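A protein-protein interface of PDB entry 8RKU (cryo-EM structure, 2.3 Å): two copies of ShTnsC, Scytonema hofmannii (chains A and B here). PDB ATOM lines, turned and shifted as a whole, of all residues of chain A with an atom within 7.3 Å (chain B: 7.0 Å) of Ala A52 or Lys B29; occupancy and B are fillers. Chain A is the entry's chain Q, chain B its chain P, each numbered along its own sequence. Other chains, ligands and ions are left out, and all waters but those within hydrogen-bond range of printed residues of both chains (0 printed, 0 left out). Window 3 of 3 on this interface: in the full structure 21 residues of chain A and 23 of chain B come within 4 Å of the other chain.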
ATOM      1  N   LEU A  46     -25.344  -1.655  15.306  1.00  0.00           N
ATOM      2  CA  LEU A  46     -24.382  -2.240  16.242  1.00  0.00           C
ATOM      3  C   LEU A  46     -24.383  -3.766  16.227  1.00  0.00           C
ATOM      4  O   LEU A  46     -23.328  -4.384  16.382  1.00  0.00           O
ATOM      5  CB  LEU A  46     -24.644  -1.744  17.664  1.00  0.00           C
ATOM      6  CG  LEU A  46     -24.331  -0.290  17.986  1.00  0.00           C
ATOM      7  CD1 LEU A  46     -24.549  -0.019  19.468  1.00  0.00           C
ATOM      8  CD2 LEU A  46     -22.904   0.022  17.592  1.00  0.00           C
ATOM      9  N   ASP A  47     -25.544  -4.396  16.059  1.00  0.00           N
ATOM     10  CA  ASP A  47     -25.548  -5.844  15.861  1.00  0.00           C
ATOM     11  C   ASP A  47     -24.859  -6.248  14.563  1.00  0.00           C
ATOM     12  O   ASP A  47     -24.101  -7.223  14.537  1.00  0.00           O
ATOM     13  CB  ASP A  47     -26.978  -6.381  15.894  1.00  0.00           C
ATOM     14  CG  ASP A  47     -27.511  -6.518  17.303  1.00  0.00           C
ATOM     15  OD1 ASP A  47     -26.691  -6.673  18.232  1.00  0.00           O
ATOM     16  OD2 ASP A  47     -28.745  -6.469  17.485  1.00  0.00           O
ATOM     17  N   GLY A  48     -25.108  -5.524  13.477  1.00  0.00           N
ATOM     18  CA  GLY A  48     -24.405  -5.818  12.240  1.00  0.00           C
ATOM     19  C   GLY A  48     -22.910  -5.593  12.340  1.00  0.00           C
ATOM     20  O   GLY A  48     -22.118  -6.350  11.771  1.00  0.00           O
ATOM     21  N   LYS A  49     -22.503  -4.552  13.067  1.00  0.00           N
ATOM     22  CA  LYS A  49     -21.085  -4.244  13.211  1.00  0.00           C
ATOM     23  C   LYS A  49     -20.382  -5.218  14.151  1.00  0.00           C
ATOM     24  O   LYS A  49     -19.272  -5.677  13.860  1.00  0.00           O
ATOM     25  CB  LYS A  49     -20.921  -2.814  13.716  1.00  0.00           C
ATOM     26  CG  LYS A  49     -19.612  -2.185  13.331  1.00  0.00           C
ATOM     27  CD  LYS A  49     -19.610  -1.840  11.857  1.00  0.00           C
ATOM     28  CE  LYS A  49     -20.626  -0.746  11.567  1.00  0.00           C
ATOM     29  NZ  LYS A  49     -20.676  -0.379  10.127  1.00  0.00           N
ATOM     30  N   ARG A  50     -21.017  -5.547  15.277  1.00  0.00           N
ATOM     31  CA  ARG A  50     -20.506  -6.582  16.172  1.00  0.00           C
ATOM     32  C   ARG A  50     -20.423  -7.939  15.480  1.00  0.00           C
ATOM     33  O   ARG A  50     -19.464  -8.688  15.688  1.00  0.00           O
ATOM     34  CB  ARG A  50     -21.377  -6.671  17.421  1.00  0.00           C
ATOM     35  CG  ARG A  50     -20.834  -7.609  18.476  1.00  0.00           C
ATOM     36  CD  ARG A  50     -21.598  -7.493  19.772  1.00  0.00           C
ATOM     37  NE  ARG A  50     -23.026  -7.726  19.605  1.00  0.00           N
ATOM     38  CZ  ARG A  50     -23.601  -8.914  19.710  1.00  0.00           C
ATOM     39  NH1 ARG A  50     -22.890 -10.007  19.927  1.00  0.00           N
ATOM     40  NH2 ARG A  50     -24.923  -9.009  19.599  1.00  0.00           N
ATOM     41  N   LYS A  51     -21.426  -8.278  14.673  1.00  0.00           N
ATOM     42  CA  LYS A  51     -21.364  -9.502  13.880  1.00  0.00           C
ATOM     43  C   LYS A  51     -20.107  -9.540  13.016  1.00  0.00           C
ATOM     44  O   LYS A  51     -19.453 -10.582  12.908  1.00  0.00           O
ATOM     45  CB  LYS A  51     -22.621  -9.609  13.016  1.00  0.00           C
ATOM     46  CG  LYS A  51     -22.733 -10.859  12.169  1.00  0.00           C
ATOM     47  CD  LYS A  51     -23.849 -10.703  11.152  1.00  0.00           C
ATOM     48  CE  LYS A  51     -25.183 -10.372  11.811  1.00  0.00           C
ATOM     49  NZ  LYS A  51     -25.761 -11.510  12.575  1.00  0.00           N
ATOM     50  N   ALA A  52     -19.756  -8.419  12.393  1.00  0.00           N
ATOM     51  CA  ALA A  52     -18.565  -8.318  11.559  1.00  0.00           C
ATOM     52  C   ALA A  52     -17.307  -7.971  12.346  1.00  0.00           C
ATOM     53  O   ALA A  52     -16.208  -8.056  11.792  1.00  0.00           O
ATOM     54  CB  ALA A  52     -18.779  -7.277  10.457  1.00  0.00           C
ATOM     55  N   ARG A  53     -17.444  -7.594  13.620  1.00  0.00           N
ATOM     56  CA  ARG A  53     -16.332  -7.167  14.476  1.00  0.00           C
ATOM     57  C   ARG A  53     -15.547  -5.997  13.887  1.00  0.00           C
ATOM     58  O   ARG A  53     -14.361  -5.826  14.177  1.00  0.00           O
ATOM     59  CB  ARG A  53     -15.390  -8.334  14.788  1.00  0.00           C
ATOM     60  CG  ARG A  53     -16.083  -9.526  15.414  1.00  0.00           C
ATOM     61  CD  ARG A  53     -16.600  -9.210  16.817  1.00  0.00           C
ATOM     62  NE  ARG A  53     -17.163 -10.391  17.464  1.00  0.00           N
ATOM     63  CZ  ARG A  53     -16.450 -11.401  17.939  1.00  0.00           C
ATOM     64  NH1 ARG A  53     -15.131 -11.350  17.992  1.00  0.00           N
ATOM     65  NH2 ARG A  53     -17.077 -12.476  18.404  1.00  0.00           N
ATOM     66  N   LYS A  54     -16.190  -5.193  13.045  1.00  0.00           N
ATOM     67  CA  LYS A  54     -15.591  -3.942  12.602  1.00  0.00           C
ATOM     68  C   LYS A  54     -15.592  -2.932  13.744  1.00  0.00           C
ATOM     69  O   LYS A  54     -16.465  -2.943  14.611  1.00  0.00           O
ATOM     70  CB  LYS A  54     -16.320  -3.387  11.381  1.00  0.00           C
ATOM     71  CG  LYS A  54     -15.636  -3.733  10.071  1.00  0.00           C
ATOM     72  CD  LYS A  54     -15.809  -5.197   9.704  1.00  0.00           C
ATOM     73  CE  LYS A  54     -15.405  -5.457   8.258  1.00  0.00           C
ATOM     74  NZ  LYS A  54     -16.250  -4.700   7.299  1.00  0.00           N
ATOM     75  N   SER A  55     -14.609  -2.042  13.727  1.00  0.00           N
ATOM     76  CA  SER A  55     -14.639  -0.823  14.522  1.00  0.00           C
ATOM     77  C   SER A  55     -15.327   0.314  13.783  1.00  0.00           C
ATOM     78  O   SER A  55     -15.358   0.356  12.550  1.00  0.00           O
ATOM     79  CB  SER A  55     -13.218  -0.405  14.901  1.00  0.00           C
ATOM     80  OG  SER A  55     -12.771  -1.091  16.055  1.00  0.00           O
ATOM     81  N   GLY A 165     -10.113  -9.507  17.909  1.00  0.00           N
ATOM     82  CA  GLY A 165     -11.193  -9.177  16.997  1.00  0.00           C
ATOM     83  C   GLY A 165     -12.367  -8.505  17.675  1.00  0.00           C
ATOM     84  O   GLY A 165     -13.471  -9.050  17.678  1.00  0.00           O
ATOM     85  N   ALA A 167     -14.972  -5.294  18.135  1.00  0.00           N
ATOM     86  CA  ALA A 167     -15.644  -4.087  17.650  1.00  0.00           C
ATOM     87  C   ALA A 167     -15.593  -2.983  18.702  1.00  0.00           C
ATOM     88  O   ALA A 167     -16.521  -2.778  19.486  1.00  0.00           O
ATOM     89  CB  ALA A 167     -17.084  -4.408  17.274  1.00  0.00           C
ATOM     90  N   GLU B  24     -19.849 -18.667   6.685  1.00  0.00           N
ATOM     91  CA  GLU B  24     -19.355 -17.581   5.841  1.00  0.00           C
ATOM     92  C   GLU B  24     -19.118 -16.303   6.635  1.00  0.00           C
ATOM     93  O   GLU B  24     -18.115 -15.615   6.425  1.00  0.00           O
ATOM     94  CB  GLU B  24     -20.326 -17.324   4.691  1.00  0.00           C
ATOM     95  CG  GLU B  24     -20.396 -18.458   3.693  1.00  0.00           C
ATOM     96  CD  GLU B  24     -19.035 -18.834   3.145  1.00  0.00           C
ATOM     97  OE1 GLU B  24     -18.345 -17.946   2.604  1.00  0.00           O
ATOM     98  OE2 GLU B  24     -18.653 -20.013   3.266  1.00  0.00           O
ATOM     99  N   ILE B  25     -20.035 -15.951   7.534  1.00  0.00           N
ATOM    100  CA  ILE B  25     -19.799 -14.814   8.419  1.00  0.00           C
ATOM    101  C   ILE B  25     -18.530 -15.011   9.245  1.00  0.00           C
ATOM    102  O   ILE B  25     -17.726 -14.082   9.405  1.00  0.00           O
ATOM    103  CB  ILE B  25     -21.026 -14.575   9.319  1.00  0.00           C
ATOM    104  CG1 ILE B  25     -22.189 -14.028   8.489  1.00  0.00           C
ATOM    105  CG2 ILE B  25     -20.682 -13.617  10.449  1.00  0.00           C
ATOM    106  CD1 ILE B  25     -23.540 -14.234   9.117  1.00  0.00           C
ATOM    107  N   ALA B  26     -18.319 -16.221   9.766  1.00  0.00           N
ATOM    108  CA  ALA B  26     -17.133 -16.480  10.577  1.00  0.00           C
ATOM    109  C   ALA B  26     -15.823 -16.304   9.812  1.00  0.00           C
ATOM    110  O   ALA B  26     -14.816 -15.904  10.409  1.00  0.00           O
ATOM    111  CB  ALA B  26     -17.207 -17.890  11.163  1.00  0.00           C
ATOM    112  N   ARG B  27     -15.800 -16.588   8.508  1.00  0.00           N
ATOM    113  CA  ARG B  27     -14.630 -16.229   7.708  1.00  0.00           C
ATOM    114  C   ARG B  27     -14.619 -14.760   7.283  1.00  0.00           C
ATOM    115  O   ARG B  27     -13.556 -14.131   7.260  1.00  0.00           O
ATOM    116  CB  ARG B  27     -14.513 -17.157   6.494  1.00  0.00           C
ATOM    117  CG  ARG B  27     -15.726 -17.209   5.595  1.00  0.00           C
ATOM    118  CD  ARG B  27     -15.524 -18.165   4.437  1.00  0.00           C
ATOM    119  NE  ARG B  27     -14.602 -17.641   3.438  1.00  0.00           N
ATOM    120  CZ  ARG B  27     -14.982 -17.012   2.337  1.00  0.00           C
ATOM    121  NH1 ARG B  27     -16.261 -16.868   2.030  1.00  0.00           N
ATOM    122  NH2 ARG B  27     -14.059 -16.537   1.508  1.00  0.00           N
ATOM    123  N   LEU B  28     -15.779 -14.193   6.945  1.00  0.00           N
ATOM    124  CA  LEU B  28     -15.807 -12.808   6.485  1.00  0.00           C
ATOM    125  C   LEU B  28     -15.503 -11.809   7.594  1.00  0.00           C
ATOM    126  O   LEU B  28     -15.038 -10.700   7.309  1.00  0.00           O
ATOM    127  CB  LEU B  28     -17.156 -12.501   5.841  1.00  0.00           C
ATOM    128  CG  LEU B  28     -17.396 -13.193   4.499  1.00  0.00           C
ATOM    129  CD1 LEU B  28     -18.861 -13.119   4.081  1.00  0.00           C
ATOM    130  CD2 LEU B  28     -16.504 -12.568   3.444  1.00  0.00           C
ATOM    131  N   LYS B  29     -15.768 -12.156   8.851  1.00  0.00           N
ATOM    132  CA  LYS B  29     -15.319 -11.301   9.944  1.00  0.00           C
ATOM    133  C   LYS B  29     -13.836 -11.483  10.259  1.00  0.00           C
ATOM    134  O   LYS B  29     -13.299 -10.736  11.085  1.00  0.00           O
ATOM    135  CB  LYS B  29     -16.205 -11.506  11.188  1.00  0.00           C
ATOM    136  CG  LYS B  29     -16.141 -12.837  11.929  1.00  0.00           C
ATOM    137  CD  LYS B  29     -14.988 -12.896  12.919  1.00  0.00           C
ATOM    138  CE  LYS B  29     -14.979 -14.208  13.680  1.00  0.00           C
ATOM    139  NZ  LYS B  29     -13.768 -14.342  14.534  1.00  0.00           N
ATOM    140  N   GLY B  30     -13.171 -12.457   9.639  1.00  0.00           N
ATOM    141  CA  GLY B  30     -11.754 -12.668   9.843  1.00  0.00           C
ATOM    142  C   GLY B  30     -10.886 -11.760   8.985  1.00  0.00           C
ATOM    143  O   GLY B  30     -11.357 -10.862   8.286  1.00  0.00           O
ATOM    144  N   LYS B  31      -9.580 -12.013   9.055  1.00  0.00           N
ATOM    145  CA  LYS B  31      -8.563 -11.331   8.263  1.00  0.00           C
ATOM    146  C   LYS B  31      -7.741 -12.333   7.460  1.00  0.00           C
ATOM    147  O   LYS B  31      -7.539 -13.474   7.885  1.00  0.00           O
ATOM    148  CB  LYS B  31      -7.640 -10.488   9.155  1.00  0.00           C
ATOM    149  CG  LYS B  31      -8.369  -9.417   9.946  1.00  0.00           C
ATOM    150  CD  LYS B  31      -7.416  -8.550  10.746  1.00  0.00           C
ATOM    151  CE  LYS B  31      -6.523  -9.395  11.645  1.00  0.00           C
ATOM    152  NZ  LYS B  31      -5.702  -8.568  12.572  1.00  0.00           N
ATOM    153  N   ARG B 249     -16.052  -6.941   2.761  1.00  0.00           N
ATOM    154  CA  ARG B 249     -16.492  -7.781   3.872  1.00  0.00           C
ATOM    155  C   ARG B 249     -17.751  -7.250   4.547  1.00  0.00           C
ATOM    156  O   ARG B 249     -18.573  -8.043   5.019  1.00  0.00           O
ATOM    157  CB  ARG B 249     -15.367  -7.928   4.894  1.00  0.00           C
ATOM    158  CG  ARG B 249     -14.171  -8.708   4.394  1.00  0.00           C
ATOM    159  CD  ARG B 249     -13.072  -8.730   5.440  1.00  0.00           C
ATOM    160  NE  ARG B 249     -11.785  -9.123   4.880  1.00  0.00           N
ATOM    161  CZ  ARG B 249     -11.290 -10.350   4.954  1.00  0.00           C
ATOM    162  NH1 ARG B 249     -11.910 -11.305   5.626  1.00  0.00           N
ATOM    163  NH2 ARG B 249     -10.130 -10.620   4.362  1.00  0.00           N
ATOM    164  N   GLU B 250     -17.922  -5.930   4.621  1.00  0.00           N
ATOM    165  CA  GLU B 250     -19.169  -5.378   5.139  1.00  0.00           C
ATOM    166  C   GLU B 250     -20.343  -5.721   4.228  1.00  0.00           C
ATOM    167  O   GLU B 250     -21.384  -6.201   4.689  1.00  0.00           O
ATOM    168  CB  GLU B 250     -19.033  -3.863   5.290  1.00  0.00           C
ATOM    169  CG  GLU B 250     -20.072  -3.183   6.170  1.00  0.00           C
ATOM    170  CD  GLU B 250     -19.775  -3.303   7.649  1.00  0.00           C
ATOM    171  OE1 GLU B 250     -18.863  -4.070   8.015  1.00  0.00           O
ATOM    172  OE2 GLU B 250     -20.444  -2.615   8.447  1.00  0.00           O
ATOM    173  N   ILE B 253     -21.102  -9.675   4.168  1.00  0.00           N
ATOM    174  CA  ILE B 253     -21.822 -10.120   5.358  1.00  0.00           C
ATOM    175  C   ILE B 253     -23.272  -9.659   5.320  1.00  0.00           C
ATOM    176  O   ILE B 253     -24.187 -10.413   5.671  1.00  0.00           O
ATOM    177  CB  ILE B 253     -21.105  -9.638   6.635  1.00  0.00           C
ATOM    178  CG1 ILE B 253     -19.846 -10.474   6.876  1.00  0.00           C
ATOM    179  CG2 ILE B 253     -22.043  -9.694   7.838  1.00  0.00           C
ATOM    180  CD1 ILE B 253     -18.992 -10.002   8.023  1.00  0.00           C
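O of Lys A49 is in hydrogen-bond range of N of Lys A54 (3.2 Å).
Among the printed residues, merely in contact across the chains: Lys A51 with Ile B25, Lys A51 with Lys B29, Lys A51 with Ile B253, Ala A52 with Lys B29 and Ala A52 with Ile B253.
Of the 11 printed residues of chain B, 4 touch a printed residue of chain A.
Among the printed residues, 7 pairs touch across the chains.
Among the printed residues, Asp or Glu carboxylates within 4 Å of a Lys or Arg side-chain nitrogen of the other chain: Lys A49 with Glu B250 and Lys A54 with Glu B250.
NZ of Lys A49 lies within salt-bridge range of OE2 of Glu B250 (2.8 Å).
The side-chain carboxylate of Glu B250 lies within salt-bridge range of the side-chain amino group of Lys A54.
Of the printed residues of chain B, Lys A51 touches Ile B25, Lys B29 and Ile B253.
Ala A52 touches just these residues of chain B: Lys B29 and Ile B253.
Printed residues of chain A within 4 Å of Ile B25: Lys A51 (3.8 Å).
Ala B26 touches none of the printed residues of chain A.
Arg B27 touches none of the printed residues of chain A.
Lys B29 touches two residues of chain A.
The nearest residue of chain B that does not touch Ala A52 is Glu B250 (4.03 Å).
No position is printed for both chains.
Of the 7 pairs that touch across the chains among the printed residues, none has its exchanged pair printed and touching as well.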
